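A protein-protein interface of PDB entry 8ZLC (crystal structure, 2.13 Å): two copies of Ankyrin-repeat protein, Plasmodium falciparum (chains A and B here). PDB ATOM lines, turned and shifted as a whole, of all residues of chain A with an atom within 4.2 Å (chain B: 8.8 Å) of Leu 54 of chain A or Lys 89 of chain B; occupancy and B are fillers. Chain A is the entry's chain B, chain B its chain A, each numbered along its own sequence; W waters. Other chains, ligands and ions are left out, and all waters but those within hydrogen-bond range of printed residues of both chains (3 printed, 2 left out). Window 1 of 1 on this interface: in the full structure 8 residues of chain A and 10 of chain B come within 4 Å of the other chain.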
ATOM      1  N   GLU A  11      27.521   4.086 -31.280  1.00  0.00           N
ATOM      2  CA  GLU A  11      26.828   5.181 -30.563  1.00  0.00           C
ATOM      3  C   GLU A  11      27.795   5.817 -29.555  1.00  0.00           C
ATOM      4  O   GLU A  11      27.580   6.985 -29.240  1.00  0.00           O
ATOM      5  CB  GLU A  11      25.529   4.677 -29.929  1.00  0.00           C
ATOM      6  CG  GLU A  11      25.711   3.823 -28.686  1.00  0.00           C
ATOM      7  CD  GLU A  11      25.806   2.324 -28.904  1.00  0.00           C
ATOM      8  OE1 GLU A  11      26.448   1.900 -29.884  1.00  0.00           O
ATOM      9  OE2 GLU A  11      25.229   1.585 -28.089  1.00  0.00           O
ATOM     10  N   ASP A  12      28.801   5.071 -29.074  1.00  0.00           N
ATOM     11  CA  ASP A  12      29.832   5.564 -28.117  1.00  0.00           C
ATOM     12  C   ASP A  12      30.648   6.664 -28.803  1.00  0.00           C
ATOM     13  O   ASP A  12      30.863   7.725 -28.202  1.00  0.00           O
ATOM     14  CB  ASP A  12      30.697   4.415 -27.576  1.00  0.00           C
ATOM     15  CG  ASP A  12      29.944   3.347 -26.776  1.00  0.00           C
ATOM     16  OD1 ASP A  12      28.794   3.626 -26.311  1.00  0.00           O
ATOM     17  OD2 ASP A  12      30.495   2.232 -26.612  1.00  0.00           O
ATOM     18  N   VAL A  14      29.720   8.407 -31.641  1.00  0.00           N
ATOM     19  CA  VAL A  14      28.779   9.499 -32.024  1.00  0.00           C
ATOM     20  C   VAL A  14      28.338  10.281 -30.773  1.00  0.00           C
ATOM     21  O   VAL A  14      28.319  11.509 -30.848  1.00  0.00           O
ATOM     22  CB  VAL A  14      27.612   8.968 -32.876  1.00  0.00           C
ATOM     23  CG1 VAL A  14      26.567  10.034 -33.155  1.00  0.00           C
ATOM     24  CG2 VAL A  14      28.129   8.407 -34.189  1.00  0.00           C
ATOM     25  N   SER A  15      28.116   9.659 -29.620  1.00  0.00           N
ATOM     26  CA  SER A  15      27.696  10.410 -28.400  1.00  0.00           C
ATOM     27  C   SER A  15      28.751  11.446 -27.997  1.00  0.00           C
ATOM     28  O   SER A  15      28.355  12.520 -27.481  1.00  0.00           O
ATOM     29  CB  SER A  15      27.361   9.512 -27.238  1.00  0.00           C
ATOM     30  OG  SER A  15      28.539   9.038 -26.614  1.00  0.00           O
ATOM     31  N   MET A  50      22.010   8.996 -37.132  1.00  0.00           N
ATOM     32  CA  MET A  50      22.498   8.568 -35.792  1.00  0.00           C
ATOM     33  C   MET A  50      22.443   9.761 -34.828  1.00  0.00           C
ATOM     34  O   MET A  50      22.071   9.559 -33.664  1.00  0.00           O
ATOM     35  CB  MET A  50      23.920   8.005 -35.835  1.00  0.00           C
ATOM     36  CG  MET A  50      24.273   7.182 -34.600  1.00  0.00           C
ATOM     37  SD  MET A  50      23.389   5.562 -34.621  1.00  0.00           S
ATOM     38  CE  MET A  50      23.646   5.079 -32.918  1.00  0.00           C
ATOM     39  N   ALA A  51      22.799  10.958 -35.274  1.00  0.00           N
ATOM     40  CA  ALA A  51      22.710  12.177 -34.449  1.00  0.00           C
ATOM     41  C   ALA A  51      21.257  12.389 -33.969  1.00  0.00           C
ATOM     42  O   ALA A  51      21.057  12.669 -32.761  1.00  0.00           O
ATOM     43  CB  ALA A  51      23.263  13.357 -35.214  1.00  0.00           C
ATOM     44  N   ILE A  52      20.266  12.249 -34.843  1.00  0.00           N
ATOM     45  CA  ILE A  52      18.825  12.317 -34.439  1.00  0.00           C
ATOM     46  C   ILE A  52      18.482  11.202 -33.431  1.00  0.00           C
ATOM     47  O   ILE A  52      17.832  11.504 -32.443  1.00  0.00           O
ATOM     48  CB  ILE A  52      17.903  12.247 -35.671  1.00  0.00           C
ATOM     49  CG1 ILE A  52      18.016  13.509 -36.511  1.00  0.00           C
ATOM     50  CG2 ILE A  52      16.447  11.979 -35.267  1.00  0.00           C
ATOM     51  CD1 ILE A  52      17.685  13.256 -37.967  1.00  0.00           C
ATOM     52  N   LEU A  53      18.880   9.949 -33.667  1.00  0.00           N
ATOM     53  CA  LEU A  53      18.560   8.835 -32.730  1.00  0.00           C
ATOM     54  C   LEU A  53      19.164   9.082 -31.338  1.00  0.00           C
ATOM     55  O   LEU A  53      18.519   8.718 -30.353  1.00  0.00           O
ATOM     56  CB  LEU A  53      19.074   7.520 -33.289  1.00  0.00           C
ATOM     57  CG  LEU A  53      18.278   6.959 -34.448  1.00  0.00           C
ATOM     58  CD1 LEU A  53      18.995   5.746 -35.009  1.00  0.00           C
ATOM     59  CD2 LEU A  53      16.881   6.574 -34.001  1.00  0.00           C
ATOM     60  N   LEU A  54      20.319   9.734 -31.252  1.00  0.00           N
ATOM     61  CA  LEU A  54      21.007  10.038 -29.971  1.00  0.00           C
ATOM     62  C   LEU A  54      20.749  11.483 -29.499  1.00  0.00           C
ATOM     63  O   LEU A  54      21.313  11.838 -28.474  1.00  0.00           O
ATOM     64  CB  LEU A  54      22.502   9.771 -30.169  1.00  0.00           C
ATOM     65  CG  LEU A  54      22.866   8.321 -30.495  1.00  0.00           C
ATOM     66  CD1 LEU A  54      24.349   8.174 -30.811  1.00  0.00           C
ATOM     67  CD2 LEU A  54      22.494   7.385 -29.356  1.00  0.00           C
ATOM     68  N   ASN A  55      19.885  12.265 -30.160  1.00  0.00           N
ATOM     69  CA  ASN A  55      19.452  13.604 -29.676  1.00  0.00           C
ATOM     70  C   ASN A  55      20.681  14.513 -29.516  1.00  0.00           C
ATOM     71  O   ASN A  55      20.825  15.147 -28.456  1.00  0.00           O
ATOM     72  CB  ASN A  55      18.649  13.488 -28.371  1.00  0.00           C
ATOM     73  CG  ASN A  55      18.018  14.782 -27.899  1.00  0.00           C
ATOM     74  OD1 ASN A  55      17.653  15.641 -28.697  1.00  0.00           O
ATOM     75  ND2 ASN A  55      17.838  14.913 -26.594  1.00  0.00           N
ATOM     76  N   LYS A  56      21.557  14.536 -30.517  1.00  0.00           N
ATOM     77  CA  LYS A  56      22.753  15.415 -30.557  1.00  0.00           C
ATOM     78  C   LYS A  56      22.356  16.713 -31.259  1.00  0.00           C
ATOM     79  O   LYS A  56      22.659  16.858 -32.479  1.00  0.00           O
ATOM     80  CB  LYS A  56      23.913  14.721 -31.279  1.00  0.00           C
ATOM     81  CG  LYS A  56      24.332  13.379 -30.698  1.00  0.00           C
ATOM     82  CD  LYS A  56      25.067  13.475 -29.384  1.00  0.00           C
ATOM     83  CE  LYS A  56      26.420  14.140 -29.531  1.00  0.00           C
ATOM     84  NZ  LYS A  56      26.880  14.669 -28.227  1.00  0.00           N
ATOM     85  N   ILE B  52      12.555  11.219 -19.849  1.00  0.00           N
ATOM     86  CA  ILE B  52      13.990  11.083 -20.224  1.00  0.00           C
ATOM     87  C   ILE B  52      14.140  10.071 -21.365  1.00  0.00           C
ATOM     88  O   ILE B  52      14.799  10.424 -22.345  1.00  0.00           O
ATOM     89  CB  ILE B  52      14.854  10.708 -19.005  1.00  0.00           C
ATOM     90  CG1 ILE B  52      14.868  11.839 -17.981  1.00  0.00           C
ATOM     91  CG2 ILE B  52      16.252  10.320 -19.462  1.00  0.00           C
ATOM     92  CD1 ILE B  52      15.194  11.397 -16.601  1.00  0.00           C
ATOM     93  N   LEU B  53      13.556   8.875 -21.237  1.00  0.00           N
ATOM     94  CA  LEU B  53      13.609   7.791 -22.254  1.00  0.00           C
ATOM     95  C   LEU B  53      13.088   8.312 -23.615  1.00  0.00           C
ATOM     96  O   LEU B  53      13.579   7.842 -24.635  1.00  0.00           O
ATOM     97  CB  LEU B  53      12.739   6.637 -21.746  1.00  0.00           C
ATOM     98  CG  LEU B  53      13.363   5.277 -21.397  1.00  0.00           C
ATOM     99  CD1 LEU B  53      14.869   5.305 -21.260  1.00  0.00           C
ATOM    100  CD2 LEU B  53      12.722   4.722 -20.146  1.00  0.00           C
ATOM    101  N   ASN B  55      12.921  11.680 -24.547  1.00  0.00           N
ATOM    102  CA  ASN B  55      13.544  12.986 -24.899  1.00  0.00           C
ATOM    103  C   ASN B  55      12.497  14.106 -24.896  1.00  0.00           C
ATOM    104  O   ASN B  55      12.563  14.983 -25.775  1.00  0.00           O
ATOM    105  CB  ASN B  55      14.286  12.907 -26.241  1.00  0.00           C
ATOM    106  CG  ASN B  55      15.534  12.032 -26.199  1.00  0.00           C
ATOM    107  OD1 ASN B  55      16.202  11.896 -25.166  1.00  0.00           O
ATOM    108  ND2 ASN B  55      15.888  11.440 -27.331  1.00  0.00           N
ATOM    109  N   LEU B  82      18.792   9.205 -13.039  1.00  0.00           N
ATOM    110  CA  LEU B  82      20.234   9.429 -13.356  1.00  0.00           C
ATOM    111  C   LEU B  82      20.779   8.249 -14.172  1.00  0.00           C
ATOM    112  O   LEU B  82      21.482   8.505 -15.162  1.00  0.00           O
ATOM    113  CB  LEU B  82      21.050   9.610 -12.072  1.00  0.00           C
ATOM    114  CG  LEU B  82      22.550   9.792 -12.331  1.00  0.00           C
ATOM    115  CD1 LEU B  82      22.816  11.068 -13.121  1.00  0.00           C
ATOM    116  CD2 LEU B  82      23.335   9.816 -11.021  1.00  0.00           C
ATOM    117  N   MET B  83      20.497   7.015 -13.738  1.00  0.00           N
ATOM    118  CA  MET B  83      20.951   5.753 -14.396  1.00  0.00           C
ATOM    119  C   MET B  83      20.467   5.689 -15.839  1.00  0.00           C
ATOM    120  O   MET B  83      21.278   5.380 -16.718  1.00  0.00           O
ATOM    121  CB  MET B  83      20.395   4.515 -13.703  1.00  0.00           C
ATOM    122  CG  MET B  83      21.169   4.126 -12.480  1.00  0.00           C
ATOM    123  SD  MET B  83      20.470   2.610 -11.755  1.00  0.00           S
ATOM    124  CE  MET B  83      20.814   2.941 -10.031  1.00  0.00           C
ATOM    125  N   ILE B  84      19.170   5.933 -16.039  1.00  0.00           N
ATOM    126  CA  ILE B  84      18.493   5.919 -17.362  1.00  0.00           C
ATOM    127  C   ILE B  84      19.101   7.015 -18.232  1.00  0.00           C
ATOM    128  O   ILE B  84      19.351   6.735 -19.414  1.00  0.00           O
ATOM    129  CB  ILE B  84      16.968   6.068 -17.160  1.00  0.00           C
ATOM    130  CG1 ILE B  84      16.377   4.767 -16.609  1.00  0.00           C
ATOM    131  CG2 ILE B  84      16.272   6.517 -18.441  1.00  0.00           C
ATOM    132  CD1 ILE B  84      15.031   4.924 -15.910  1.00  0.00           C
ATOM    133  N   ALA B  85      19.272   8.228 -17.687  1.00  0.00           N
ATOM    134  CA  ALA B  85      19.852   9.373 -18.408  1.00  0.00           C
ATOM    135  C   ALA B  85      21.255   8.985 -18.901  1.00  0.00           C
ATOM    136  O   ALA B  85      21.553   9.235 -20.099  1.00  0.00           O
ATOM    137  CB  ALA B  85      19.881  10.607 -17.537  1.00  0.00           C
ATOM    138  N   CYS B  86      22.092   8.403 -18.034  1.00  0.00           N
ATOM    139  CA  CYS B  86      23.463   7.984 -18.410  1.00  0.00           C
ATOM    140  C   CYS B  86      23.379   6.874 -19.457  1.00  0.00           C
ATOM    141  O   CYS B  86      24.107   6.976 -20.468  1.00  0.00           O
ATOM    142  CB  CYS B  86      24.295   7.530 -17.216  1.00  0.00           C
ATOM    143  SG  CYS B  86      24.715   8.916 -16.125  1.00  0.00           S
ATOM    144  N   ASP B  87      22.531   5.862 -19.242  1.00  0.00           N
ATOM    145  CA  ASP B  87      22.446   4.704 -20.156  1.00  0.00           C
ATOM    146  C   ASP B  87      22.053   5.188 -21.569  1.00  0.00           C
ATOM    147  O   ASP B  87      22.647   4.674 -22.527  1.00  0.00           O
ATOM    148  CB  ASP B  87      21.513   3.628 -19.596  1.00  0.00           C
ATOM    149  CG  ASP B  87      21.434   2.376 -20.458  1.00  0.00           C
ATOM    150  OD1 ASP B  87      22.402   1.590 -20.446  1.00  0.00           O
ATOM    151  OD2 ASP B  87      20.424   2.224 -21.179  1.00  0.00           O
ATOM    152  N   LYS B  88      21.104   6.127 -21.706  1.00  0.00           N
ATOM    153  CA  LYS B  88      20.615   6.627 -23.023  1.00  0.00           C
ATOM    154  C   LYS B  88      21.482   7.762 -23.565  1.00  0.00           C
ATOM    155  O   LYS B  88      21.178   8.186 -24.649  1.00  0.00           O
ATOM    156  CB  LYS B  88      19.179   7.161 -22.965  1.00  0.00           C
ATOM    157  CG  LYS B  88      18.124   6.106 -22.692  1.00  0.00           C
ATOM    158  CD  LYS B  88      18.235   4.859 -23.553  1.00  0.00           C
ATOM    159  CE  LYS B  88      17.695   3.638 -22.841  1.00  0.00           C
ATOM    160  NZ  LYS B  88      17.740   2.441 -23.707  1.00  0.00           N
ATOM    161  N   LYS B  89      22.533   8.201 -22.877  1.00  0.00           N
ATOM    162  CA  LYS B  89      23.471   9.222 -23.409  1.00  0.00           C
ATOM    163  C   LYS B  89      22.655  10.447 -23.831  1.00  0.00           C
ATOM    164  O   LYS B  89      22.807  10.947 -24.966  1.00  0.00           O
ATOM    165  CB  LYS B  89      24.300   8.621 -24.539  1.00  0.00           C
ATOM    166  CG  LYS B  89      24.932   7.281 -24.179  1.00  0.00           C
ATOM    167  CD  LYS B  89      24.750   6.237 -25.250  1.00  0.00           C
ATOM    168  CE  LYS B  89      25.416   4.911 -24.921  1.00  0.00           C
ATOM    169  NZ  LYS B  89      26.893   5.015 -24.978  1.00  0.00           N
ATOM    170  N   VAL B  90      21.811  10.913 -22.923  1.00  0.00           N
ATOM    171  CA  VAL B  90      21.000  12.147 -23.106  1.00  0.00           C
ATOM    172  C   VAL B  90      21.988  13.297 -22.943  1.00  0.00           C
ATOM    173  O   VAL B  90      23.121  13.061 -22.524  1.00  0.00           O
ATOM    174  CB  VAL B  90      19.796  12.179 -22.133  1.00  0.00           C
ATOM    175  CG1 VAL B  90      18.985  10.901 -22.234  1.00  0.00           C
ATOM    176  CG2 VAL B  90      20.209  12.426 -20.687  1.00  0.00           C
ATOM    177  N   PRO B  91      21.631  14.553 -23.304  1.00  0.00           N
ATOM    178  CA  PRO B  91      22.567  15.674 -23.216  1.00  0.00           C
ATOM    179  C   PRO B  91      23.144  15.856 -21.807  1.00  0.00           C
ATOM    180  O   PRO B  91      22.439  15.633 -20.837  1.00  0.00           O
ATOM    181  CB  PRO B  91      21.725  16.900 -23.609  1.00  0.00           C
ATOM    182  CG  PRO B  91      20.634  16.302 -24.483  1.00  0.00           C
ATOM    183  CD  PRO B  91      20.325  14.965 -23.833  1.00  0.00           C
ATOM    184  N   LEU B  92      24.397  16.289 -21.739  1.00  0.00           N
ATOM    185  CA  LEU B  92      25.167  16.397 -20.482  1.00  0.00           C
ATOM    186  C   LEU B  92      24.480  17.386 -19.527  1.00  0.00           C
ATOM    187  O   LEU B  92      24.560  17.154 -18.293  1.00  0.00           O
ATOM    188  CB  LEU B  92      26.596  16.826 -20.825  1.00  0.00           C
ATOM    189  CG  LEU B  92      27.601  16.681 -19.689  1.00  0.00           C
ATOM    190  CD1 LEU B  92      27.731  15.213 -19.265  1.00  0.00           C
ATOM    191  CD2 LEU B  92      28.957  17.258 -20.099  1.00  0.00           C
ATOM    192  N   TRP B  94      21.250  17.820 -18.985  1.00  0.00           N
ATOM    193  CA  TRP B  94      20.163  17.096 -18.253  1.00  0.00           C
ATOM    194  C   TRP B  94      20.775  16.265 -17.123  1.00  0.00           C
ATOM    195  O   TRP B  94      20.208  16.268 -16.009  1.00  0.00           O
ATOM    196  CB  TRP B  94      19.345  16.165 -19.141  1.00  0.00           C
ATOM    197  CG  TRP B  94      18.677  16.794 -20.321  1.00  0.00           C
ATOM    198  CD1 TRP B  94      18.847  18.052 -20.847  1.00  0.00           C
ATOM    199  CD2 TRP B  94      17.761  16.113 -21.187  1.00  0.00           C
ATOM    200  NE1 TRP B  94      18.091  18.191 -21.981  1.00  0.00           N
ATOM    201  CE2 TRP B  94      17.421  17.017 -22.220  1.00  0.00           C
ATOM    202  CE3 TRP B  94      17.236  14.815 -21.211  1.00  0.00           C
ATOM    203  CZ2 TRP B  94      16.556  16.660 -23.248  1.00  0.00           C
ATOM    204  CZ3 TRP B  94      16.354  14.479 -22.214  1.00  0.00           C
ATOM    205  CH2 TRP B  94      16.021  15.392 -23.221  1.00  0.00           C
ATOM    206  N   ILE B  95      21.877  15.574 -17.413  1.00  0.00           N
ATOM    207  CA  ILE B  95      22.591  14.782 -16.380  1.00  0.00           C
ATOM    208  C   ILE B  95      23.005  15.750 -15.267  1.00  0.00           C
ATOM    209  O   ILE B  95      22.660  15.476 -14.105  1.00  0.00           O
ATOM    210  CB  ILE B  95      23.744  13.959 -16.977  1.00  0.00           C
ATOM    211  CG1 ILE B  95      23.234  12.989 -18.043  1.00  0.00           C
ATOM    212  CG2 ILE B  95      24.483  13.203 -15.890  1.00  0.00           C
ATOM    213  CD1 ILE B  95      24.327  12.423 -18.923  1.00  0.00           C
ATOM    214  N   LYS B 120      27.074   2.765 -16.158  1.00  0.00           N
ATOM    215  CA  LYS B 120      26.319   2.903 -17.439  1.00  0.00           C
ATOM    216  C   LYS B 120      26.976   3.955 -18.348  1.00  0.00           C
ATOM    217  O   LYS B 120      26.570   4.038 -19.505  1.00  0.00           O
ATOM    218  CB  LYS B 120      24.853   3.304 -17.233  1.00  0.00           C
ATOM    219  CG  LYS B 120      24.119   2.654 -16.075  1.00  0.00           C
ATOM    220  CD  LYS B 120      23.588   1.286 -16.326  1.00  0.00           C
ATOM    221  CE  LYS B 120      22.473   0.965 -15.342  1.00  0.00           C
ATOM    222  NZ  LYS B 120      21.829  -0.326 -15.651  1.00  0.00           N
ATOM    223  N   CYS B 121      27.916   4.758 -17.849  1.00  0.00           N
ATOM    224  CA  CYS B 121      28.700   5.706 -18.686  1.00  0.00           C
ATOM    225  C   CYS B 121      29.829   4.948 -19.391  1.00  0.00           C
ATOM    226  O   CYS B 121      30.349   3.994 -18.815  1.00  0.00           O
ATOM    227  CB  CYS B 121      29.300   6.825 -17.859  1.00  0.00           C
ATOM    228  SG  CYS B 121      28.065   7.777 -16.954  1.00  0.00           S
ATOM    229  N   ASN B 122      30.196   5.369 -20.586  1.00  0.00           N
ATOM    230  CA  ASN B 122      31.366   4.815 -21.310  1.00  0.00           C
ATOM    231  C   ASN B 122      32.656   5.331 -20.672  1.00  0.00           C
ATOM    232  O   ASN B 122      32.717   6.540 -20.314  1.00  0.00           O
ATOM    233  CB  ASN B 122      31.392   5.231 -22.783  1.00  0.00           C
ATOM    234  CG  ASN B 122      30.336   4.533 -23.600  1.00  0.00           C
ATOM    235  OD1 ASN B 122      30.209   3.308 -23.550  1.00  0.00           O
ATOM    236  ND2 ASN B 122      29.590   5.320 -24.357  1.00  0.00           N
ATOM    237  N   PHE B 123      33.663   4.462 -20.619  1.00  0.00           N
ATOM    238  CA  PHE B 123      35.078   4.814 -20.337  1.00  0.00           C
ATOM    239  C   PHE B 123      35.406   6.203 -20.911  1.00  0.00           C
ATOM    240  O   PHE B 123      35.286   6.406 -22.148  1.00  0.00           O
ATOM    241  CB  PHE B 123      36.025   3.735 -20.882  1.00  0.00           C
ATOM    242  N   SER B 125      34.121   9.043 -21.027  1.00  0.00           N
ATOM    243  CA  SER B 125      33.078   9.913 -21.629  1.00  0.00           C
ATOM    244  C   SER B 125      33.005  11.213 -20.837  1.00  0.00           C
ATOM    245  O   SER B 125      33.500  11.253 -19.687  1.00  0.00           O
ATOM    246  CB  SER B 125      31.748   9.210 -21.706  1.00  0.00           C
ATOM    247  OG  SER B 125      31.213   8.950 -20.419  1.00  0.00           O
ATOM    248  N   ALA B 127      30.266  12.176 -19.655  1.00  0.00           N
ATOM    249  CA  ALA B 127      29.298  11.802 -18.593  1.00  0.00           C
ATOM    250  C   ALA B 127      30.061  11.248 -17.377  1.00  0.00           C
ATOM    251  O   ALA B 127      29.810  11.716 -16.230  1.00  0.00           O
ATOM    252  CB  ALA B 127      28.289  10.808 -19.139  1.00  0.00           C
HETATM  253  O   HOH W   1      31.215   7.512 -25.400  1.00  0.00           O
HETATM  254  O   HOH W   2      16.331  11.174 -30.245  1.00  0.00           O
HETATM  255  O   HOH W   3      29.359   8.529 -24.155  1.00  0.00           O
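CG of Glu 11 of chain A touches CE of Lys 89 of chain B (3.9 Å).
O of Lys 89 of chain B touches O of Leu 54 of chain A (3.9 Å).
ND2 of Asn 55 of chain B touches CB of Asn 55 of chain A (3.6 Å).
Asn 55 of chain A touches Pro 91 of chain B (ND2 to CD, 3.7 Å).
CH2 of Trp 94 of chain B touches ND2 of Asn 55 of chain A (3.9 Å).
Asn 55 of chain A touches its own counterpart, Asn 55 of chain B.
3 positions are printed for both chains.
Of the 7 pairs that touch across the chains among the printed residues, 1 has its exchanged pair printed and touching as well.
The side-chain amide oxygen (OD1) of Asn 55 of chain B lies close to the backbone carbonyl oxygen (O) of Ile 52 of chain B (3.5 Å).
ND2 of Asn 122 of chain B lies close to NZ of Lys 89 of chain B (2.8 Å).
OG of Ser 125 of chain B sits at hydrogen-bond distance from O of Asn 122 of chain B.
The backbone carbonyl oxygen (O) of Glu 11 of chain A sits close to the side-chain hydroxyl (OG) of Ser 15 of chain A, at 3.5 Å.
O of Asp 12 of chain A lies within hydrogen-bond range of OG of Ser 15 of chain A.
Along chain A the printed residues that touch a printed residue of chain B span positions 11 to 55.
Of the 22 printed residues of chain B, 5 touch a printed residue of chain A.
Hydrophobic or aromatic side chains of chain B within 4 Å of the printed part of chain A: Pro 91 and Trp 94.
Among the printed residues, 7 pairs touch across the chains.
Among the printed residues, Asp or Glu carboxylates within 4 Å of a Lys or Arg side-chain nitrogen of the other chain: Asp 12 of chain A with Lys 89 of chain B.
Of the printed residues of chain B, Asp 12 of chain A touches Lys 89 (2.7 Å) and Asn 122 (2.7 Å).
Of chain B, only Lys 89 comes within 4 Å of Leu 54 of chain A.
Of the printed residues of chain A, Lys 89 of chain B touches Glu 11 (3.9 Å), Asp 12 (2.7 Å) and Leu 54 (3.9 Å).
Printed residues of chain A within 4 Å of Asn 122 of chain B: Asp 12 (2.7 Å).
The nearest printed residue of chain A that does not touch Lys 89 of chain B is Ser 15 of chain A (4.2 Å).
The nearest printed residue of chain A that does not touch Pro 91 of chain B is Leu 54 of chain A (5.7 Å).
The side-chain carboxylate (OD1) of Asp 12 of chain A is in salt-bridge range of the side-chain amino group (NZ) of Lys 89 of chain B.
The side-chain carboxylate (OD1) of Asp 12 of chain A sits at hydrogen-bond distance from the side-chain amide nitrogen (ND2) of Asn 122 of chain B, 2.7 Å away.
Water W3 bridges the side-chain hydroxyl of Ser 15 of chain A (2.6 Å) and the side-chain amide nitrogen of Asn 122 of chain B (3.2 Å).
Water W2 lies within hydrogen-bond range of the backbone carbonyl oxygen of Ile 52 of chain A (2.7 Å), the side-chain amide nitrogen of Asn 55 of chain B (3.0 Å) and the backbone carbonyl oxygen of Leu 53 of chain A (3.3 Å).
Water W1 lies within hydrogen-bond range of O of Asp 12 of chain A (2.8 Å), ND2 of Asn 122 of chain B (2.9 Å) and OG of Ser 15 of chain A (3.3 Å).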
